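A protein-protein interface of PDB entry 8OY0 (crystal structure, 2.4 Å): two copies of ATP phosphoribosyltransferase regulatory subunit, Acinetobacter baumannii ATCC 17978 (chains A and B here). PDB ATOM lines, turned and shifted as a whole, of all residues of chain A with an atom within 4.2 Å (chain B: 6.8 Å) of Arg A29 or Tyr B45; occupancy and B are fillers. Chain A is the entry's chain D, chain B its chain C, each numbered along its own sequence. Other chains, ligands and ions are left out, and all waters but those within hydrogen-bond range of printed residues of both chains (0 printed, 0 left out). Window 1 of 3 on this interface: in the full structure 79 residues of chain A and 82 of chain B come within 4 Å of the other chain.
The backbone NH (N) of Val A17 is in hydrogen-bond range of the backbone carbonyl oxygen (O) of Tyr B45, at 3.0 Å.
The guanidinium group (NH2) of Arg B29 is in salt-bridge range of the side-chain carboxylate (OE2) of Glu A26, at 2.9 Å.
The side-chain hydroxyl (OH) of Tyr B45 lies within hydrogen-bond range of the guanidinium group (NH1) of Arg A29.
OH of Tyr B45 is in hydrogen-bond range of OE1 of Glu A26 (2.6 Å).
OE2 of Glu B26 is in salt-bridge range of NH2 of Arg B29 (3.5 Å).
The guanidinium group (NH2) of Arg A29 lies within hydrogen-bond range of the backbone carbonyl oxygen (O) of Ala A110, at 3.2 Å.
The side-chain carboxylate (OE2) of Glu A26 is in salt-bridge range of the guanidinium group (NE) of Arg A30, 2.8 Å away.
N of Val B44 sits at hydrogen-bond distance from O of Cys B108 (3.0 Å).
OE2 of Glu B26 is in salt-bridge range of NE of Arg B30, 2.8 Å away.
O of Tyr B45 touches CA of Asp A16 (3.8 Å).
Asp A16 touches Pro B47 (OD1 to CD, 3.2 Å).
Ile B94 touches Asp A16 (CD1 to OD1, 3.5 Å).
Val B44 touches Val A17 (CA to O, 3.3 Å).
Leu B43 touches Glu A26.
Arg A29 touches Arg B29.
Arg B30 touches Arg A30 (O to NH2, 3.6 Å).
CG2 of Ile A33 touches NH2 of Arg B30, at 3.8 Å.
Tyr A321 touches Tyr B45 (OH to CD2, 3.8 Å).
Printed residues of chain B within 4 Å of Asp A16: Tyr B45 (3.8 Å), Pro B47 (3.2 Å) and Ile B94 (3.5 Å).
Arg A29 touches just these residues of chain B: Arg B29 (3.6 Å) and Tyr B45 (3.3 Å).
Of the printed residues of chain B, Ile A33 touches Arg B30 (3.8 Å).
Of the printed residues of chain B, Tyr A321 touches Tyr B45.
Printed residues of chain A within 4 Å of Tyr B45: Asp A16, Val A17, Glu A26, Arg A29 and Tyr A321.
The nearest residue of chain A that does not touch Tyr B45 is Ile A25 (4.1 Å).
The nearest printed residue of chain B that does not touch Glu A26 is Arg B30 (4.9 Å).
Hydrophobic or aromatic side chains of chain A that line the printed part of chain B: Val A17, Ile A33 and Tyr A321.
Of the 14 printed residues of chain B, 7 touch a printed residue of chain A.
Printed residues of chain B that touch a printed residue of chain A: Arg B29, Arg B30, Leu B43, Val B44, Tyr B45, Pro B47 and Ile B94.
Hydrophobic or aromatic side chains of chain B within 4 Å of the printed part of chain A: Leu B43, Val B44, Tyr B45, Pro B47 and Ile B94.
Among the printed residues, Asp or Glu carboxylates within 4 Å of a Lys or Arg side-chain nitrogen of the other chain: Glu A26 with Arg B29 (2.9 Å).
Glu A26 touches Arg B29, but with the chains exchanged Arg A29 does not touch Glu B26 (5.2 Å).
Arg A29 touches its own counterpart, Arg B29.
Arg A30 touches its own counterpart, Arg B30.
Positions printed for both chains: 26, 29, 30 and 110.
Of the 13 pairs that touch across the chains among the printed residues, 2 have their exchanged pair printed and touching as well.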
ATOM      1  N   ASP A  16      24.844  -4.382  40.992  1.00  0.00           N
ATOM      2  CA  ASP A  16      24.183  -4.706  39.743  1.00  0.00           C
ATOM      3  C   ASP A  16      23.382  -3.491  39.291  1.00  0.00           C
ATOM      4  O   ASP A  16      22.901  -2.721  40.126  1.00  0.00           O
ATOM      5  CB  ASP A  16      23.256  -5.911  39.918  1.00  0.00           C
ATOM      6  CG  ASP A  16      23.969  -7.147  40.441  1.00  0.00           C
ATOM      7  OD1 ASP A  16      24.964  -7.555  39.802  1.00  0.00           O
ATOM      8  OD2 ASP A  16      23.518  -7.703  41.469  1.00  0.00           O
ATOM      9  N   VAL A  17      23.274  -3.319  37.968  1.00  0.00           N
ATOM     10  CA  VAL A  17      22.244  -2.468  37.402  1.00  0.00           C
ATOM     11  C   VAL A  17      21.191  -3.400  36.818  1.00  0.00           C
ATOM     12  O   VAL A  17      21.375  -3.988  35.745  1.00  0.00           O
ATOM     13  CB  VAL A  17      22.785  -1.487  36.345  1.00  0.00           C
ATOM     14  CG1 VAL A  17      21.697  -0.534  35.865  1.00  0.00           C
ATOM     15  CG2 VAL A  17      23.976  -0.708  36.869  1.00  0.00           C
ATOM     16  N   ILE A  25      19.071   3.959  32.009  1.00  0.00           N
ATOM     17  CA  ILE A  25      20.445   4.400  31.801  1.00  0.00           C
ATOM     18  C   ILE A  25      20.878   4.143  30.351  1.00  0.00           C
ATOM     19  O   ILE A  25      21.550   4.985  29.749  1.00  0.00           O
ATOM     20  CB  ILE A  25      21.394   3.739  32.823  1.00  0.00           C
ATOM     21  CG1 ILE A  25      21.040   4.111  34.265  1.00  0.00           C
ATOM     22  CG2 ILE A  25      22.838   4.080  32.524  1.00  0.00           C
ATOM     23  CD1 ILE A  25      21.249   5.566  34.605  1.00  0.00           C
ATOM     24  N   GLU A  26      20.494   2.981  29.798  1.00  0.00           N
ATOM     25  CA  GLU A  26      20.848   2.602  28.436  1.00  0.00           C
ATOM     26  C   GLU A  26      20.274   3.620  27.453  1.00  0.00           C
ATOM     27  O   GLU A  26      20.977   4.079  26.556  1.00  0.00           O
ATOM     28  CB  GLU A  26      20.339   1.187  28.130  1.00  0.00           C
ATOM     29  CG  GLU A  26      20.617   0.710  26.719  1.00  0.00           C
ATOM     30  CD  GLU A  26      22.084   0.523  26.378  1.00  0.00           C
ATOM     31  OE1 GLU A  26      22.898   0.383  27.305  1.00  0.00           O
ATOM     32  OE2 GLU A  26      22.410   0.533  25.169  1.00  0.00           O
ATOM     33  N   LYS A  27      18.990   3.955  27.631  1.00  0.00           N
ATOM     34  CA  LYS A  27      18.309   4.942  26.805  1.00  0.00           C
ATOM     35  C   LYS A  27      19.044   6.276  26.899  1.00  0.00           C
ATOM     36  O   LYS A  27      19.270   6.947  25.888  1.00  0.00           O
ATOM     37  CB  LYS A  27      16.859   5.063  27.279  1.00  0.00           C
ATOM     38  CG  LYS A  27      15.926   5.943  26.457  1.00  0.00           C
ATOM     39  CD  LYS A  27      14.621   6.206  27.185  1.00  0.00           C
ATOM     40  CE  LYS A  27      13.511   6.680  26.272  1.00  0.00           C
ATOM     41  NZ  LYS A  27      13.758   8.048  25.784  1.00  0.00           N
ATOM     42  N   LEU A  28      19.430   6.631  28.125  1.00  0.00           N
ATOM     43  CA  LEU A  28      20.113   7.882  28.412  1.00  0.00           C
ATOM     44  C   LEU A  28      21.489   7.904  27.743  1.00  0.00           C
ATOM     45  O   LEU A  28      21.903   8.930  27.202  1.00  0.00           O
ATOM     46  CB  LEU A  28      20.221   7.996  29.937  1.00  0.00           C
ATOM     47  CG  LEU A  28      20.253   9.400  30.522  1.00  0.00           C
ATOM     48  CD1 LEU A  28      18.956  10.136  30.237  1.00  0.00           C
ATOM     49  CD2 LEU A  28      20.477   9.332  32.025  1.00  0.00           C
ATOM     50  N   ARG A  29      22.178   6.753  27.790  1.00  0.00           N
ATOM     51  CA  ARG A  29      23.496   6.580  27.200  1.00  0.00           C
ATOM     52  C   ARG A  29      23.429   6.803  25.689  1.00  0.00           C
ATOM     53  O   ARG A  29      24.227   7.552  25.143  1.00  0.00           O
ATOM     54  CB  ARG A  29      23.998   5.165  27.520  1.00  0.00           C
ATOM     55  CG  ARG A  29      25.440   4.852  27.151  1.00  0.00           C
ATOM     56  CD  ARG A  29      25.577   3.395  26.739  1.00  0.00           C
ATOM     57  NE  ARG A  29      26.919   2.877  26.935  1.00  0.00           N
ATOM     58  CZ  ARG A  29      27.286   2.106  27.958  1.00  0.00           C
ATOM     59  NH1 ARG A  29      26.460   1.891  28.973  1.00  0.00           N
ATOM     60  NH2 ARG A  29      28.504   1.583  27.983  1.00  0.00           N
ATOM     61  N   ARG A  30      22.468   6.150  25.026  1.00  0.00           N
ATOM     62  CA  ARG A  30      22.372   6.187  23.574  1.00  0.00           C
ATOM     63  C   ARG A  30      22.066   7.608  23.098  1.00  0.00           C
ATOM     64  O   ARG A  30      22.681   8.099  22.150  1.00  0.00           O
ATOM     65  CB  ARG A  30      21.286   5.230  23.073  1.00  0.00           C
ATOM     66  CG  ARG A  30      21.569   3.762  23.341  1.00  0.00           C
ATOM     67  CD  ARG A  30      20.450   2.874  22.826  1.00  0.00           C
ATOM     68  NE  ARG A  30      20.646   1.476  23.178  1.00  0.00           N
ATOM     69  CZ  ARG A  30      19.959   0.456  22.668  1.00  0.00           C
ATOM     70  NH1 ARG A  30      19.054   0.672  21.729  1.00  0.00           N
ATOM     71  NH2 ARG A  30      20.192  -0.779  23.083  1.00  0.00           N
ATOM     72  N   GLU A  31      21.103   8.257  23.761  1.00  0.00           N
ATOM     73  CA  GLU A  31      20.639   9.566  23.331  1.00  0.00           C
ATOM     74  C   GLU A  31      21.738  10.611  23.530  1.00  0.00           C
ATOM     75  O   GLU A  31      21.845  11.555  22.743  1.00  0.00           O
ATOM     76  CB  GLU A  31      19.357   9.940  24.073  1.00  0.00           C
ATOM     77  CG  GLU A  31      18.147   9.131  23.628  1.00  0.00           C
ATOM     78  CD  GLU A  31      16.844   9.514  24.312  1.00  0.00           C
ATOM     79  OE1 GLU A  31      16.836  10.519  25.040  1.00  0.00           O
ATOM     80  OE2 GLU A  31      15.833   8.819  24.102  1.00  0.00           O
ATOM     81  N   ALA A  32      22.552  10.432  24.578  1.00  0.00           N
ATOM     82  CA  ALA A  32      23.656  11.336  24.854  1.00  0.00           C
ATOM     83  C   ALA A  32      24.740  11.178  23.786  1.00  0.00           C
ATOM     84  O   ALA A  32      25.233  12.166  23.254  1.00  0.00           O
ATOM     85  CB  ALA A  32      24.203  11.084  26.246  1.00  0.00           C
ATOM     86  N   ILE A  33      25.117   9.931  23.491  1.00  0.00           N
ATOM     87  CA  ILE A  33      26.096   9.657  22.452  1.00  0.00           C
ATOM     88  C   ILE A  33      25.617  10.284  21.142  1.00  0.00           C
ATOM     89  O   ILE A  33      26.397  10.926  20.442  1.00  0.00           O
ATOM     90  CB  ILE A  33      26.340   8.142  22.300  1.00  0.00           C
ATOM     91  CG1 ILE A  33      26.937   7.519  23.563  1.00  0.00           C
ATOM     92  CG2 ILE A  33      27.193   7.841  21.075  1.00  0.00           C
ATOM     93  CD1 ILE A  33      28.120   8.268  24.102  1.00  0.00           C
ATOM     94  N   ALA A 110      31.565   6.808  26.533  1.00  0.00           N
ATOM     95  CA  ALA A 110      30.589   6.496  27.564  1.00  0.00           C
ATOM     96  C   ALA A 110      30.829   5.080  28.075  1.00  0.00           C
ATOM     97  O   ALA A 110      30.452   4.113  27.418  1.00  0.00           O
ATOM     98  CB  ALA A 110      29.190   6.646  27.025  1.00  0.00           C
ATOM     99  N   LEU A 128      29.524   5.542  35.583  1.00  0.00           N
ATOM    100  CA  LEU A 128      29.445   5.450  34.135  1.00  0.00           C
ATOM    101  C   LEU A 128      29.817   6.812  33.552  1.00  0.00           C
ATOM    102  O   LEU A 128      28.998   7.728  33.507  1.00  0.00           O
ATOM    103  CB  LEU A 128      28.025   4.998  33.769  1.00  0.00           C
ATOM    104  CG  LEU A 128      27.679   4.926  32.280  1.00  0.00           C
ATOM    105  CD1 LEU A 128      28.749   4.213  31.473  1.00  0.00           C
ATOM    106  CD2 LEU A 128      26.344   4.222  32.079  1.00  0.00           C
ATOM    107  N   LEU A 320      26.810   9.355  34.404  1.00  0.00           N
ATOM    108  CA  LEU A 320      25.510   9.198  33.774  1.00  0.00           C
ATOM    109  C   LEU A 320      24.453   8.805  34.808  1.00  0.00           C
ATOM    110  O   LEU A 320      23.283   9.123  34.631  1.00  0.00           O
ATOM    111  CB  LEU A 320      25.608   8.156  32.650  1.00  0.00           C
ATOM    112  CG  LEU A 320      25.583   8.704  31.222  1.00  0.00           C
ATOM    113  CD1 LEU A 320      25.463   7.580  30.205  1.00  0.00           C
ATOM    114  CD2 LEU A 320      24.445   9.702  31.038  1.00  0.00           C
ATOM    115  N   TYR A 321      24.861   8.132  35.890  1.00  0.00           N
ATOM    116  CA  TYR A 321      23.930   7.744  36.938  1.00  0.00           C
ATOM    117  C   TYR A 321      23.378   8.983  37.652  1.00  0.00           C
ATOM    118  O   TYR A 321      22.287   8.921  38.215  1.00  0.00           O
ATOM    119  CB  TYR A 321      24.570   6.761  37.927  1.00  0.00           C
ATOM    120  CG  TYR A 321      24.978   5.443  37.312  1.00  0.00           C
ATOM    121  CD1 TYR A 321      24.052   4.640  36.663  1.00  0.00           C
ATOM    122  CD2 TYR A 321      26.291   4.997  37.362  1.00  0.00           C
ATOM    123  CE1 TYR A 321      24.420   3.432  36.086  1.00  0.00           C
ATOM    124  CE2 TYR A 321      26.671   3.790  36.797  1.00  0.00           C
ATOM    125  CZ  TYR A 321      25.733   3.004  36.152  1.00  0.00           C
ATOM    126  OH  TYR A 321      26.090   1.818  35.562  1.00  0.00           O
ATOM    127  N   GLU B  26      29.011  -0.249  17.832  1.00  0.00           N
ATOM    128  CA  GLU B  26      27.974   0.377  18.638  1.00  0.00           C
ATOM    129  C   GLU B  26      26.602   0.062  18.049  1.00  0.00           C
ATOM    130  O   GLU B  26      25.689  -0.321  18.773  1.00  0.00           O
ATOM    131  CB  GLU B  26      28.202   1.891  18.729  1.00  0.00           C
ATOM    132  CG  GLU B  26      27.133   2.629  19.524  1.00  0.00           C
ATOM    133  CD  GLU B  26      27.086   2.299  21.008  1.00  0.00           C
ATOM    134  OE1 GLU B  26      28.092   1.778  21.538  1.00  0.00           O
ATOM    135  OE2 GLU B  26      26.040   2.549  21.631  1.00  0.00           O
ATOM    136  N   ARG B  29      25.892  -3.491  18.674  1.00  0.00           N
ATOM    137  CA  ARG B  29      25.601  -3.675  20.088  1.00  0.00           C
ATOM    138  C   ARG B  29      24.137  -3.348  20.370  1.00  0.00           C
ATOM    139  O   ARG B  29      23.440  -4.125  21.004  1.00  0.00           O
ATOM    140  CB  ARG B  29      26.521  -2.784  20.927  1.00  0.00           C
ATOM    141  CG  ARG B  29      26.530  -3.131  22.407  1.00  0.00           C
ATOM    142  CD  ARG B  29      27.235  -2.094  23.251  1.00  0.00           C
ATOM    143  NE  ARG B  29      26.473  -0.855  23.357  1.00  0.00           N
ATOM    144  CZ  ARG B  29      25.710  -0.511  24.394  1.00  0.00           C
ATOM    145  NH1 ARG B  29      25.443  -1.386  25.351  1.00  0.00           N
ATOM    146  NH2 ARG B  29      25.188   0.704  24.451  1.00  0.00           N
ATOM    147  N   ARG B  30      23.677  -2.195  19.887  1.00  0.00           N
ATOM    148  CA  ARG B  30      22.327  -1.722  20.164  1.00  0.00           C
ATOM    149  C   ARG B  30      21.293  -2.659  19.550  1.00  0.00           C
ATOM    150  O   ARG B  30      20.312  -3.011  20.200  1.00  0.00           O
ATOM    151  CB  ARG B  30      22.122  -0.303  19.626  1.00  0.00           C
ATOM    152  CG  ARG B  30      22.982   0.747  20.311  1.00  0.00           C
ATOM    153  CD  ARG B  30      22.716   2.135  19.764  1.00  0.00           C
ATOM    154  NE  ARG B  30      23.598   3.143  20.342  1.00  0.00           N
ATOM    155  CZ  ARG B  30      23.523   4.446  20.082  1.00  0.00           C
ATOM    156  NH1 ARG B  30      22.589   4.923  19.276  1.00  0.00           N
ATOM    157  NH2 ARG B  30      24.410   5.271  20.613  1.00  0.00           N
ATOM    158  N   LEU B  43      17.884  -6.384  29.652  1.00  0.00           N
ATOM    159  CA  LEU B  43      19.259  -5.944  29.780  1.00  0.00           C
ATOM    160  C   LEU B  43      19.589  -5.696  31.250  1.00  0.00           C
ATOM    161  O   LEU B  43      18.782  -5.122  31.982  1.00  0.00           O
ATOM    162  CB  LEU B  43      19.433  -4.662  28.959  1.00  0.00           C
ATOM    163  CG  LEU B  43      20.806  -3.999  29.032  1.00  0.00           C
ATOM    164  CD1 LEU B  43      21.858  -4.862  28.350  1.00  0.00           C
ATOM    165  CD2 LEU B  43      20.774  -2.619  28.406  1.00  0.00           C
ATOM    166  N   VAL B  44      20.778  -6.156  31.662  1.00  0.00           N
ATOM    167  CA  VAL B  44      21.369  -5.813  32.941  1.00  0.00           C
ATOM    168  C   VAL B  44      22.814  -5.400  32.672  1.00  0.00           C
ATOM    169  O   VAL B  44      23.393  -5.809  31.674  1.00  0.00           O
ATOM    170  CB  VAL B  44      21.296  -6.976  33.953  1.00  0.00           C
ATOM    171  CG1 VAL B  44      19.874  -7.488  34.140  1.00  0.00           C
ATOM    172  CG2 VAL B  44      22.212  -8.128  33.581  1.00  0.00           C
ATOM    173  N   TYR B  45      23.363  -4.549  33.542  1.00  0.00           N
ATOM    174  CA  TYR B  45      24.802  -4.365  33.634  1.00  0.00           C
ATOM    175  C   TYR B  45      25.296  -5.103  34.870  1.00  0.00           C
ATOM    176  O   TYR B  45      24.811  -4.862  35.977  1.00  0.00           O
ATOM    177  CB  TYR B  45      25.197  -2.893  33.764  1.00  0.00           C
ATOM    178  CG  TYR B  45      24.724  -1.947  32.686  1.00  0.00           C
ATOM    179  CD1 TYR B  45      24.325  -2.387  31.434  1.00  0.00           C
ATOM    180  CD2 TYR B  45      24.675  -0.581  32.937  1.00  0.00           C
ATOM    181  CE1 TYR B  45      23.901  -1.493  30.457  1.00  0.00           C
ATOM    182  CE2 TYR B  45      24.245   0.321  31.980  1.00  0.00           C
ATOM    183  CZ  TYR B  45      23.858  -0.136  30.733  1.00  0.00           C
ATOM    184  OH  TYR B  45      23.451   0.794  29.807  1.00  0.00           O
ATOM    185  N   THR B  46      26.250  -6.009  34.680  1.00  0.00           N
ATOM    186  CA  THR B  46      26.863  -6.707  35.795  1.00  0.00           C
ATOM    187  C   THR B  46      28.030  -5.863  36.302  1.00  0.00           C
ATOM    188  O   THR B  46      28.550  -5.021  35.575  1.00  0.00           O
ATOM    189  CB  THR B  46      27.287  -8.130  35.401  1.00  0.00           C
ATOM    190  OG1 THR B  46      28.355  -8.080  34.452  1.00  0.00           O
ATOM    191  CG2 THR B  46      26.127  -8.933  34.857  1.00  0.00           C
ATOM    192  N   PRO B  47      28.473  -6.066  37.558  1.00  0.00           N
ATOM    193  CA  PRO B  47      29.672  -5.411  38.068  1.00  0.00           C
ATOM    194  C   PRO B  47      30.930  -5.813  37.312  1.00  0.00           C
ATOM    195  O   PRO B  47      31.072  -6.964  36.900  1.00  0.00           O
ATOM    196  CB  PRO B  47      29.801  -5.923  39.511  1.00  0.00           C
ATOM    197  CG  PRO B  47      28.425  -6.436  39.860  1.00  0.00           C
ATOM    198  CD  PRO B  47      27.852  -6.948  38.557  1.00  0.00           C
ATOM    199  N   ARG B  84      35.698  -9.180  35.973  1.00  0.00           N
ATOM    200  CA  ARG B  84      34.855 -10.181  35.350  1.00  0.00           C
ATOM    201  C   ARG B  84      35.510 -10.686  34.063  1.00  0.00           C
ATOM    202  O   ARG B  84      35.980  -9.898  33.244  1.00  0.00           O
ATOM    203  CB  ARG B  84      33.459  -9.613  35.070  1.00  0.00           C
ATOM    204  CG  ARG B  84      33.432  -8.522  34.012  1.00  0.00           C
ATOM    205  CD  ARG B  84      32.067  -7.897  33.840  1.00  0.00           C
ATOM    206  NE  ARG B  84      32.084  -6.960  32.725  1.00  0.00           N
ATOM    207  CZ  ARG B  84      31.176  -6.018  32.499  1.00  0.00           C
ATOM    208  NH1 ARG B  84      30.187  -5.825  33.360  1.00  0.00           N
ATOM    209  NH2 ARG B  84      31.280  -5.258  31.419  1.00  0.00           N
ATOM    210  N   MET B  87      30.274 -13.174  32.227  1.00  0.00           N
ATOM    211  CA  MET B  87      29.150 -12.619  32.959  1.00  0.00           C
ATOM    212  C   MET B  87      28.141 -13.701  33.338  1.00  0.00           C
ATOM    213  O   MET B  87      27.266 -13.456  34.167  1.00  0.00           O
ATOM    214  CB  MET B  87      28.490 -11.525  32.121  1.00  0.00           C
ATOM    215  CG  MET B  87      29.456 -10.375  31.871  1.00  0.00           C
ATOM    216  SD  MET B  87      28.664  -8.894  31.262  1.00  0.00           S
ATOM    217  CE  MET B  87      29.461  -8.762  29.664  1.00  0.00           C
ATOM    218  N   ILE B  94      22.368 -12.944  40.166  1.00  0.00           N
ATOM    219  CA  ILE B  94      21.225 -12.047  40.122  1.00  0.00           C
ATOM    220  C   ILE B  94      19.933 -12.861  40.199  1.00  0.00           C
ATOM    221  O   ILE B  94      19.049 -12.547  41.000  1.00  0.00           O
ATOM    222  CB  ILE B  94      21.297 -11.146  38.874  1.00  0.00           C
ATOM    223  CG1 ILE B  94      22.390 -10.083  39.036  1.00  0.00           C
ATOM    224  CG2 ILE B  94      19.946 -10.528  38.560  1.00  0.00           C
ATOM    225  CD1 ILE B  94      22.702  -9.312  37.780  1.00  0.00           C
ATOM    226  N   CYS B 108      19.819 -10.385  29.527  1.00  0.00           N
ATOM    227  CA  CYS B 108      20.946 -10.310  28.615  1.00  0.00           C
ATOM    228  C   CYS B 108      21.924  -9.230  29.072  1.00  0.00           C
ATOM    229  O   CYS B 108      21.619  -8.442  29.956  1.00  0.00           O
ATOM    230  CB  CYS B 108      20.494 -10.072  27.177  1.00  0.00           C
ATOM    231  SG  CYS B 108      19.800  -8.426  26.871  1.00  0.00           S
ATOM    232  N   TYR B 109      23.110  -9.242  28.457  1.00  0.00           N
ATOM    233  CA  TYR B 109      24.203  -8.353  28.816  1.00  0.00           C
ATOM    234  C   TYR B 109      25.067  -8.117  27.584  1.00  0.00           C
ATOM    235  O   TYR B 109      25.070  -8.933  26.673  1.00  0.00           O
ATOM    236  CB  TYR B 109      25.018  -8.961  29.960  1.00  0.00           C
ATOM    237  CG  TYR B 109      25.306 -10.432  29.789  1.00  0.00           C
ATOM    238  CD1 TYR B 109      26.366 -10.882  29.020  1.00  0.00           C
ATOM    239  CD2 TYR B 109      24.477 -11.384  30.362  1.00  0.00           C
ATOM    240  CE1 TYR B 109      26.615 -12.235  28.851  1.00  0.00           C
ATOM    241  CE2 TYR B 109      24.713 -12.739  30.212  1.00  0.00           C
ATOM    242  CZ  TYR B 109      25.782 -13.168  29.446  1.00  0.00           C
ATOM    243  OH  TYR B 109      25.993 -14.515  29.291  1.00  0.00           O
ATOM    244  N   ALA B 110      25.794  -6.999  27.581  1.00  0.00           N
ATOM    245  CA  ALA B 110      26.756  -6.698  26.536  1.00  0.00           C
ATOM    246  C   ALA B 110      27.817  -5.757  27.091  1.00  0.00           C
ATOM    247  O   ALA B 110      27.579  -4.562  27.221  1.00  0.00           O
ATOM    248  CB  ALA B 110      26.078  -6.086  25.339  1.00  0.00           C
